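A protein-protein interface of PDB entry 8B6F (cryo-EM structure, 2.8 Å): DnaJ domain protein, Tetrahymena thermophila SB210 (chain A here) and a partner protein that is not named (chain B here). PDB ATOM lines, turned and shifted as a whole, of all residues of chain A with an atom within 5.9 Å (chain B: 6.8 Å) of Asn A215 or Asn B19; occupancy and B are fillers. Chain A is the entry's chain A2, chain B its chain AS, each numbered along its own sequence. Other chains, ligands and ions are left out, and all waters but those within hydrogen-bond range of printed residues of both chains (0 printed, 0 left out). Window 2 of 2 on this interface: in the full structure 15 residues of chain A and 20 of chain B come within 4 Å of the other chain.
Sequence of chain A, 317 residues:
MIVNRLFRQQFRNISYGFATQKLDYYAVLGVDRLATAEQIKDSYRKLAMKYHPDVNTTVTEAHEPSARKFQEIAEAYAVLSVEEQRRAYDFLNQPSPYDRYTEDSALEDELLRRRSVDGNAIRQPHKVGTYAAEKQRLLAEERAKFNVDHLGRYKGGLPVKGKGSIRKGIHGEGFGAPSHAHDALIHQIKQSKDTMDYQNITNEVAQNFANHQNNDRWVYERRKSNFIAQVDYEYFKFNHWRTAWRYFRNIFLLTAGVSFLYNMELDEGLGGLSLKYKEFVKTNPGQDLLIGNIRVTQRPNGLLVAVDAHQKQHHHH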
ATOM      1  N   ASN A 208     -24.532  -9.765 -23.973  1.00  0.00           N
ATOM      2  CA  ASN A 208     -24.812  -9.370 -22.597  1.00  0.00           C
ATOM      3  C   ASN A 208     -25.684 -10.407 -21.905  1.00  0.00           C
ATOM      4  O   ASN A 208     -25.449 -10.750 -20.741  1.00  0.00           O
ATOM      5  CB  ASN A 208     -25.485  -8.000 -22.563  1.00  0.00           C
ATOM      6  CG  ASN A 208     -24.594  -6.898 -23.094  1.00  0.00           C
ATOM      7  OD1 ASN A 208     -23.371  -7.024 -23.109  1.00  0.00           O
ATOM      8  ND2 ASN A 208     -25.205  -5.801 -23.522  1.00  0.00           N
ATOM      9  N   ALA A 210     -25.850 -13.601 -22.654  1.00  0.00           N
ATOM     10  CA  ALA A 210     -25.023 -14.783 -22.439  1.00  0.00           C
ATOM     11  C   ALA A 210     -24.084 -14.596 -21.256  1.00  0.00           C
ATOM     12  O   ALA A 210     -23.917 -15.505 -20.437  1.00  0.00           O
ATOM     13  CB  ALA A 210     -24.230 -15.104 -23.704  1.00  0.00           C
ATOM     14  N   ASN A 211     -23.463 -13.420 -21.145  1.00  0.00           N
ATOM     15  CA  ASN A 211     -22.575 -13.165 -20.016  1.00  0.00           C
ATOM     16  C   ASN A 211     -23.337 -13.213 -18.699  1.00  0.00           C
ATOM     17  O   ASN A 211     -22.839 -13.758 -17.707  1.00  0.00           O
ATOM     18  CB  ASN A 211     -21.880 -11.814 -20.179  1.00  0.00           C
ATOM     19  CG  ASN A 211     -21.058 -11.729 -21.451  1.00  0.00           C
ATOM     20  OD1 ASN A 211     -21.088 -10.721 -22.154  1.00  0.00           O
ATOM     21  ND2 ASN A 211     -20.320 -12.793 -21.754  1.00  0.00           N
ATOM     22  N   HIS A 212     -24.543 -12.648 -18.666  1.00  0.00           N
ATOM     23  CA  HIS A 212     -25.341 -12.693 -17.447  1.00  0.00           C
ATOM     24  C   HIS A 212     -25.687 -14.127 -17.067  1.00  0.00           C
ATOM     25  O   HIS A 212     -25.620 -14.499 -15.890  1.00  0.00           O
ATOM     26  CB  HIS A 212     -26.616 -11.869 -17.622  1.00  0.00           C
ATOM     27  CG  HIS A 212     -27.476 -11.828 -16.397  1.00  0.00           C
ATOM     28  ND1 HIS A 212     -27.143 -11.093 -15.279  1.00  0.00           N
ATOM     29  CD2 HIS A 212     -28.650 -12.436 -16.111  1.00  0.00           C
ATOM     30  CE1 HIS A 212     -28.077 -11.248 -14.359  1.00  0.00           C
ATOM     31  NE2 HIS A 212     -29.003 -12.058 -14.838  1.00  0.00           N
ATOM     32  N   GLN A 213     -26.063 -14.949 -18.048  1.00  0.00           N
ATOM     33  CA  GLN A 213     -26.432 -16.328 -17.750  1.00  0.00           C
ATOM     34  C   GLN A 213     -25.228 -17.160 -17.330  1.00  0.00           C
ATOM     35  O   GLN A 213     -25.371 -18.094 -16.534  1.00  0.00           O
ATOM     36  CB  GLN A 213     -27.114 -16.960 -18.962  1.00  0.00           C
ATOM     37  CG  GLN A 213     -28.417 -16.285 -19.355  1.00  0.00           C
ATOM     38  CD  GLN A 213     -29.460 -16.339 -18.259  1.00  0.00           C
ATOM     39  OE1 GLN A 213     -29.669 -17.379 -17.637  1.00  0.00           O
ATOM     40  NE2 GLN A 213     -30.115 -15.212 -18.010  1.00  0.00           N
ATOM     41  N   ASN A 214     -24.038 -16.845 -17.849  1.00  0.00           N
ATOM     42  CA  ASN A 214     -22.853 -17.620 -17.496  1.00  0.00           C
ATOM     43  C   ASN A 214     -22.561 -17.555 -16.002  1.00  0.00           C
ATOM     44  O   ASN A 214     -21.932 -18.467 -15.455  1.00  0.00           O
ATOM     45  CB  ASN A 214     -21.646 -17.130 -18.293  1.00  0.00           C
ATOM     46  CG  ASN A 214     -21.756 -17.449 -19.771  1.00  0.00           C
ATOM     47  OD1 ASN A 214     -22.792 -17.916 -20.241  1.00  0.00           O
ATOM     48  ND2 ASN A 214     -20.683 -17.199 -20.511  1.00  0.00           N
ATOM     49  N   ASN A 215     -22.997 -16.488 -15.329  1.00  0.00           N
ATOM     50  CA  ASN A 215     -22.830 -16.413 -13.880  1.00  0.00           C
ATOM     51  C   ASN A 215     -23.634 -17.500 -13.178  1.00  0.00           C
ATOM     52  O   ASN A 215     -23.160 -18.106 -12.210  1.00  0.00           O
ATOM     53  CB  ASN A 215     -23.247 -15.034 -13.370  1.00  0.00           C
ATOM     54  CG  ASN A 215     -22.306 -13.938 -13.821  1.00  0.00           C
ATOM     55  OD1 ASN A 215     -22.497 -13.335 -14.875  1.00  0.00           O
ATOM     56  ND2 ASN A 215     -21.283 -13.671 -13.017  1.00  0.00           N
ATOM     57  N   ASP A 216     -24.849 -17.758 -13.649  1.00  0.00           N
ATOM     58  CA  ASP A 216     -25.724 -18.771 -13.076  1.00  0.00           C
ATOM     59  C   ASP A 216     -25.614 -20.112 -13.789  1.00  0.00           C
ATOM     60  O   ASP A 216     -26.432 -21.001 -13.536  1.00  0.00           O
ATOM     61  CB  ASP A 216     -27.174 -18.287 -13.113  1.00  0.00           C
ATOM     62  CG  ASP A 216     -27.382 -17.010 -12.327  1.00  0.00           C
ATOM     63  OD1 ASP A 216     -26.854 -16.911 -11.200  1.00  0.00           O
ATOM     64  OD2 ASP A 216     -28.065 -16.100 -12.841  1.00  0.00           O
ATOM     65  N   ARG A 217     -24.626 -20.273 -14.672  1.00  0.00           N
ATOM     66  CA  ARG A 217     -24.475 -21.523 -15.411  1.00  0.00           C
ATOM     67  C   ARG A 217     -24.485 -22.734 -14.488  1.00  0.00           C
ATOM     68  O   ARG A 217     -25.075 -23.768 -14.817  1.00  0.00           O
ATOM     69  CB  ARG A 217     -23.182 -21.487 -16.225  1.00  0.00           C
ATOM     70  CG  ARG A 217     -22.738 -22.844 -16.750  1.00  0.00           C
ATOM     71  CD  ARG A 217     -21.558 -22.704 -17.693  1.00  0.00           C
ATOM     72  NE  ARG A 217     -21.917 -21.992 -18.914  1.00  0.00           N
ATOM     73  CZ  ARG A 217     -22.456 -22.558 -19.985  1.00  0.00           C
ATOM     74  NH1 ARG A 217     -22.724 -23.853 -20.024  1.00  0.00           N
ATOM     75  NH2 ARG A 217     -22.734 -21.805 -21.045  1.00  0.00           N
ATOM     76  N   TRP A 218     -23.830 -22.632 -13.331  1.00  0.00           N
ATOM     77  CA  TRP A 218     -23.740 -23.786 -12.442  1.00  0.00           C
ATOM     78  C   TRP A 218     -25.119 -24.244 -11.987  1.00  0.00           C
ATOM     79  O   TRP A 218     -25.397 -25.447 -11.940  1.00  0.00           O
ATOM     80  CB  TRP A 218     -22.862 -23.453 -11.236  1.00  0.00           C
ATOM     81  CG  TRP A 218     -22.727 -24.593 -10.275  1.00  0.00           C
ATOM     82  CD1 TRP A 218     -21.991 -25.725 -10.451  1.00  0.00           C
ATOM     83  CD2 TRP A 218     -23.341 -24.710  -8.985  1.00  0.00           C
ATOM     84  NE1 TRP A 218     -22.108 -26.542  -9.355  1.00  0.00           N
ATOM     85  CE2 TRP A 218     -22.931 -25.942  -8.440  1.00  0.00           C
ATOM     86  CE3 TRP A 218     -24.195 -23.893  -8.239  1.00  0.00           C
ATOM     87  CZ2 TRP A 218     -23.347 -26.378  -7.185  1.00  0.00           C
ATOM     88  CZ3 TRP A 218     -24.608 -24.328  -6.993  1.00  0.00           C
ATOM     89  CH2 TRP A 218     -24.183 -25.560  -6.477  1.00  0.00           C
ATOM     90  N   PRO B  12     -28.234  -4.984 -12.170  1.00  0.00           N
ATOM     91  CA  PRO B  12     -26.861  -5.446 -11.927  1.00  0.00           C
ATOM     92  C   PRO B  12     -26.842  -6.798 -11.230  1.00  0.00           C
ATOM     93  O   PRO B  12     -27.674  -7.086 -10.368  1.00  0.00           O
ATOM     94  CB  PRO B  12     -26.268  -4.349 -11.036  1.00  0.00           C
ATOM     95  CG  PRO B  12     -27.093  -3.151 -11.304  1.00  0.00           C
ATOM     96  CD  PRO B  12     -28.473  -3.656 -11.581  1.00  0.00           C
ATOM     97  N   ALA B  13     -25.876  -7.632 -11.615  1.00  0.00           N
ATOM     98  CA  ALA B  13     -25.745  -8.949 -11.007  1.00  0.00           C
ATOM     99  C   ALA B  13     -25.105  -8.901  -9.630  1.00  0.00           C
ATOM    100  O   ALA B  13     -25.204  -9.879  -8.882  1.00  0.00           O
ATOM    101  CB  ALA B  13     -24.927  -9.868 -11.914  1.00  0.00           C
ATOM    102  N   SER B  14     -24.453  -7.796  -9.279  1.00  0.00           N
ATOM    103  CA  SER B  14     -23.779  -7.686  -7.998  1.00  0.00           C
ATOM    104  C   SER B  14     -23.839  -6.240  -7.533  1.00  0.00           C
ATOM    105  O   SER B  14     -24.106  -5.327  -8.316  1.00  0.00           O
ATOM    106  CB  SER B  14     -22.323  -8.160  -8.092  1.00  0.00           C
ATOM    107  OG  SER B  14     -21.662  -8.048  -6.845  1.00  0.00           O
ATOM    108  N   GLN B  17     -20.598  -4.902  -9.250  1.00  0.00           N
ATOM    109  CA  GLN B  17     -20.220  -5.388 -10.570  1.00  0.00           C
ATOM    110  C   GLN B  17     -21.472  -5.639 -11.393  1.00  0.00           C
ATOM    111  O   GLN B  17     -22.587  -5.689 -10.870  1.00  0.00           O
ATOM    112  CB  GLN B  17     -19.389  -6.671 -10.481  1.00  0.00           C
ATOM    113  CG  GLN B  17     -17.928  -6.449 -10.177  1.00  0.00           C
ATOM    114  CD  GLN B  17     -17.133  -7.729 -10.251  1.00  0.00           C
ATOM    115  OE1 GLN B  17     -17.685  -8.820 -10.145  1.00  0.00           O
ATOM    116  NE2 GLN B  17     -15.828  -7.602 -10.452  1.00  0.00           N
ATOM    117  N   ASN B  18     -21.266  -5.794 -12.700  1.00  0.00           N
ATOM    118  CA  ASN B  18     -22.293  -6.268 -13.625  1.00  0.00           C
ATOM    119  C   ASN B  18     -21.818  -7.609 -14.183  1.00  0.00           C
ATOM    120  O   ASN B  18     -21.224  -7.681 -15.261  1.00  0.00           O
ATOM    121  CB  ASN B  18     -22.550  -5.250 -14.741  1.00  0.00           C
ATOM    122  CG  ASN B  18     -23.084  -3.934 -14.216  1.00  0.00           C
ATOM    123  OD1 ASN B  18     -23.611  -3.863 -13.109  1.00  0.00           O
ATOM    124  ND2 ASN B  18     -22.957  -2.882 -15.017  1.00  0.00           N
ATOM    125  N   ASN B  19     -22.077  -8.673 -13.429  1.00  0.00           N
ATOM    126  CA  ASN B  19     -21.983 -10.044 -13.917  1.00  0.00           C
ATOM    127  C   ASN B  19     -20.556 -10.552 -14.104  1.00  0.00           C
ATOM    128  O   ASN B  19     -20.370 -11.740 -14.387  1.00  0.00           O
ATOM    129  CB  ASN B  19     -22.739 -10.180 -15.243  1.00  0.00           C
ATOM    130  CG  ASN B  19     -21.809 -10.306 -16.430  1.00  0.00           C
ATOM    131  OD1 ASN B  19     -21.462 -11.409 -16.845  1.00  0.00           O
ATOM    132  ND2 ASN B  19     -21.398  -9.174 -16.982  1.00  0.00           N
ATOM    133  N   ASN B  20     -19.544  -9.703 -13.939  1.00  0.00           N
ATOM    134  CA  ASN B  20     -18.171 -10.142 -14.174  1.00  0.00           C
ATOM    135  C   ASN B  20     -17.211  -9.020 -13.805  1.00  0.00           C
ATOM    136  O   ASN B  20     -17.613  -7.873 -13.594  1.00  0.00           O
ATOM    137  CB  ASN B  20     -17.938 -10.552 -15.630  1.00  0.00           C
ATOM    138  CG  ASN B  20     -18.017 -12.046 -15.835  1.00  0.00           C
ATOM    139  OD1 ASN B  20     -17.690 -12.825 -14.944  1.00  0.00           O
ATOM    140  ND2 ASN B  20     -18.456 -12.457 -17.019  1.00  0.00           N
ATOM    141  N   TYR B  21     -15.927  -9.372 -13.747  1.00  0.00           N
ATOM    142  CA  TYR B  21     -14.854  -8.411 -13.535  1.00  0.00           C
ATOM    143  C   TYR B  21     -14.193  -7.972 -14.833  1.00  0.00           C
ATOM    144  O   TYR B  21     -13.463  -6.977 -14.833  1.00  0.00           O
ATOM    145  CB  TYR B  21     -13.789  -8.999 -12.601  1.00  0.00           C
ATOM    146  CG  TYR B  21     -12.893 -10.034 -13.245  1.00  0.00           C
ATOM    147  CD1 TYR B  21     -13.273 -11.368 -13.312  1.00  0.00           C
ATOM    148  CD2 TYR B  21     -11.658  -9.679 -13.767  1.00  0.00           C
ATOM    149  CE1 TYR B  21     -12.454 -12.315 -13.894  1.00  0.00           C
ATOM    150  CE2 TYR B  21     -10.832 -10.617 -14.351  1.00  0.00           C
ATOM    151  CZ  TYR B  21     -11.235 -11.933 -14.409  1.00  0.00           C
ATOM    152  OH  TYR B  21     -10.414 -12.869 -14.990  1.00  0.00           O
ATOM    153  N   PHE B  22     -14.426  -8.692 -15.930  1.00  0.00           N
ATOM    154  CA  PHE B  22     -13.839  -8.373 -17.221  1.00  0.00           C
ATOM    155  C   PHE B  22     -14.878  -8.030 -18.276  1.00  0.00           C
ATOM    156  O   PHE B  22     -14.505  -7.740 -19.418  1.00  0.00           O
ATOM    157  CB  PHE B  22     -12.988  -9.549 -17.720  1.00  0.00           C
ATOM    158  CG  PHE B  22     -13.770 -10.810 -17.928  1.00  0.00           C
ATOM    159  CD1 PHE B  22     -14.023 -11.664 -16.870  1.00  0.00           C
ATOM    160  CD2 PHE B  22     -14.247 -11.144 -19.182  1.00  0.00           C
ATOM    161  CE1 PHE B  22     -14.740 -12.825 -17.057  1.00  0.00           C
ATOM    162  CE2 PHE B  22     -14.968 -12.303 -19.376  1.00  0.00           C
ATOM    163  CZ  PHE B  22     -15.213 -13.146 -18.311  1.00  0.00           C
ATOM    164  N   SER B  23     -16.164  -8.058 -17.936  1.00  0.00           N
ATOM    165  CA  SER B  23     -17.220  -7.814 -18.904  1.00  0.00           C
ATOM    166  C   SER B  23     -18.400  -7.162 -18.203  1.00  0.00           C
ATOM    167  O   SER B  23     -18.522  -7.206 -16.977  1.00  0.00           O
ATOM    168  CB  SER B  23     -17.669  -9.111 -19.585  1.00  0.00           C
ATOM    169  OG  SER B  23     -16.597  -9.719 -20.279  1.00  0.00           O
ATOM    170  N   GLY B  24     -19.262  -6.545 -19.003  1.00  0.00           N
ATOM    171  CA  GLY B  24     -20.481  -5.950 -18.495  1.00  0.00           C
ATOM    172  C   GLY B  24     -21.697  -6.445 -19.246  1.00  0.00           C
ATOM    173  O   GLY B  24     -21.783  -6.289 -20.466  1.00  0.00           O
ATOM    174  N   GLY B  25     -22.641  -7.050 -18.533  1.00  0.00           N
ATOM    175  CA  GLY B  25     -23.828  -7.587 -19.172  1.00  0.00           C
ATOM    176  C   GLY B  25     -24.943  -7.767 -18.167  1.00  0.00           C
ATOM    177  O   GLY B  25     -24.733  -7.732 -16.953  1.00  0.00           O
ATOM    178  N   GLY B  26     -26.143  -7.959 -18.698  1.00  0.00           N
ATOM    179  CA  GLY B  26     -27.307  -8.162 -17.856  1.00  0.00           C
ATOM    180  C   GLY B  26     -28.466  -8.659 -18.686  1.00  0.00           C
ATOM    181  O   GLY B  26     -28.454  -8.589 -19.918  1.00  0.00           O
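ND2 of Asn A215 lies within hydrogen-bond range of O of Asn B19. OD1 of Asn B19 lies close to O of Asn A211 (2.9 Å). The backbone carbonyl oxygen of Gly B24 lies close to the side-chain amide oxygen of Asn A208 (3.2 Å).
The side-chain amide oxygen (OD1) of Asn B19 is in hydrogen-bond range of the side-chain amide nitrogen (ND2) of Asn B20 (3.2 Å). The side-chain amide nitrogen (ND2) of Asn B19 sits close to the backbone NH (N) of Gly B25, at 2.9 Å. The backbone carbonyl oxygen (O) of Asn A211 sits close to the side-chain amide oxygen (OD1) of Asn A215, 2.9 Å away. ND2 of Asn B19 is in hydrogen-bond range of O of Ser B23, 3.5 Å away. The backbone carbonyl oxygen (O) of His A212 sits close to the side-chain amide oxygen (OD1) of Asn A215, at 3.5 Å.
Among the printed residues, merely in contact across the chains: Asn A208 with Gly B26 (3.5 Å), His A212 with Gly B26 (3.8 Å), His A212 with Asn B19 (3.8 Å) and Asn A208 with Gly B25 (3.8 Å).
Asn A215 touches just one residue of chain B: Asn B19 (2.5 Å). Asn B19 touches just these residues of chain A: Asn A211 (2.9 Å), His A212 (3.8 Å) and Asn A215 (2.5 Å). Printed residues of chain B within 4 Å of His A212: Asn B19 and Gly B26. Of the printed residues of chain A, Gly B24 touches Asn A208 (3.2 Å). Printed residues of chain B within 4 Å of Asn A208: Gly B24 (3.2 Å), Gly B25 (3.8 Å) and Gly B26 (3.5 Å). Printed residues of chain A within 4 Å of Gly B26: Asn A208 and His A212. Printed residues of chain A within 4 Å of Gly B25: Asn A208 (3.8 Å). Ser B23 touches none of the printed residues of chain A. Tyr B21 touches none of the printed residues of chain A. The nearest residue of chain B that does not touch Asn A215 is Asn B20 (4.2 Å). The nearest printed residue of chain A that does not touch Gly B24 is Asn A211 (4.8 Å).
Hydrophobic or aromatic side chains of chain A within 4 Å of the printed part of chain B: His A212. Among the printed residues, 7 pairs touch across the chains. Among the printed residues, no Asp or Glu carboxylate lies within 4 Å of a Lys or Arg side-chain nitrogen of the other chain.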
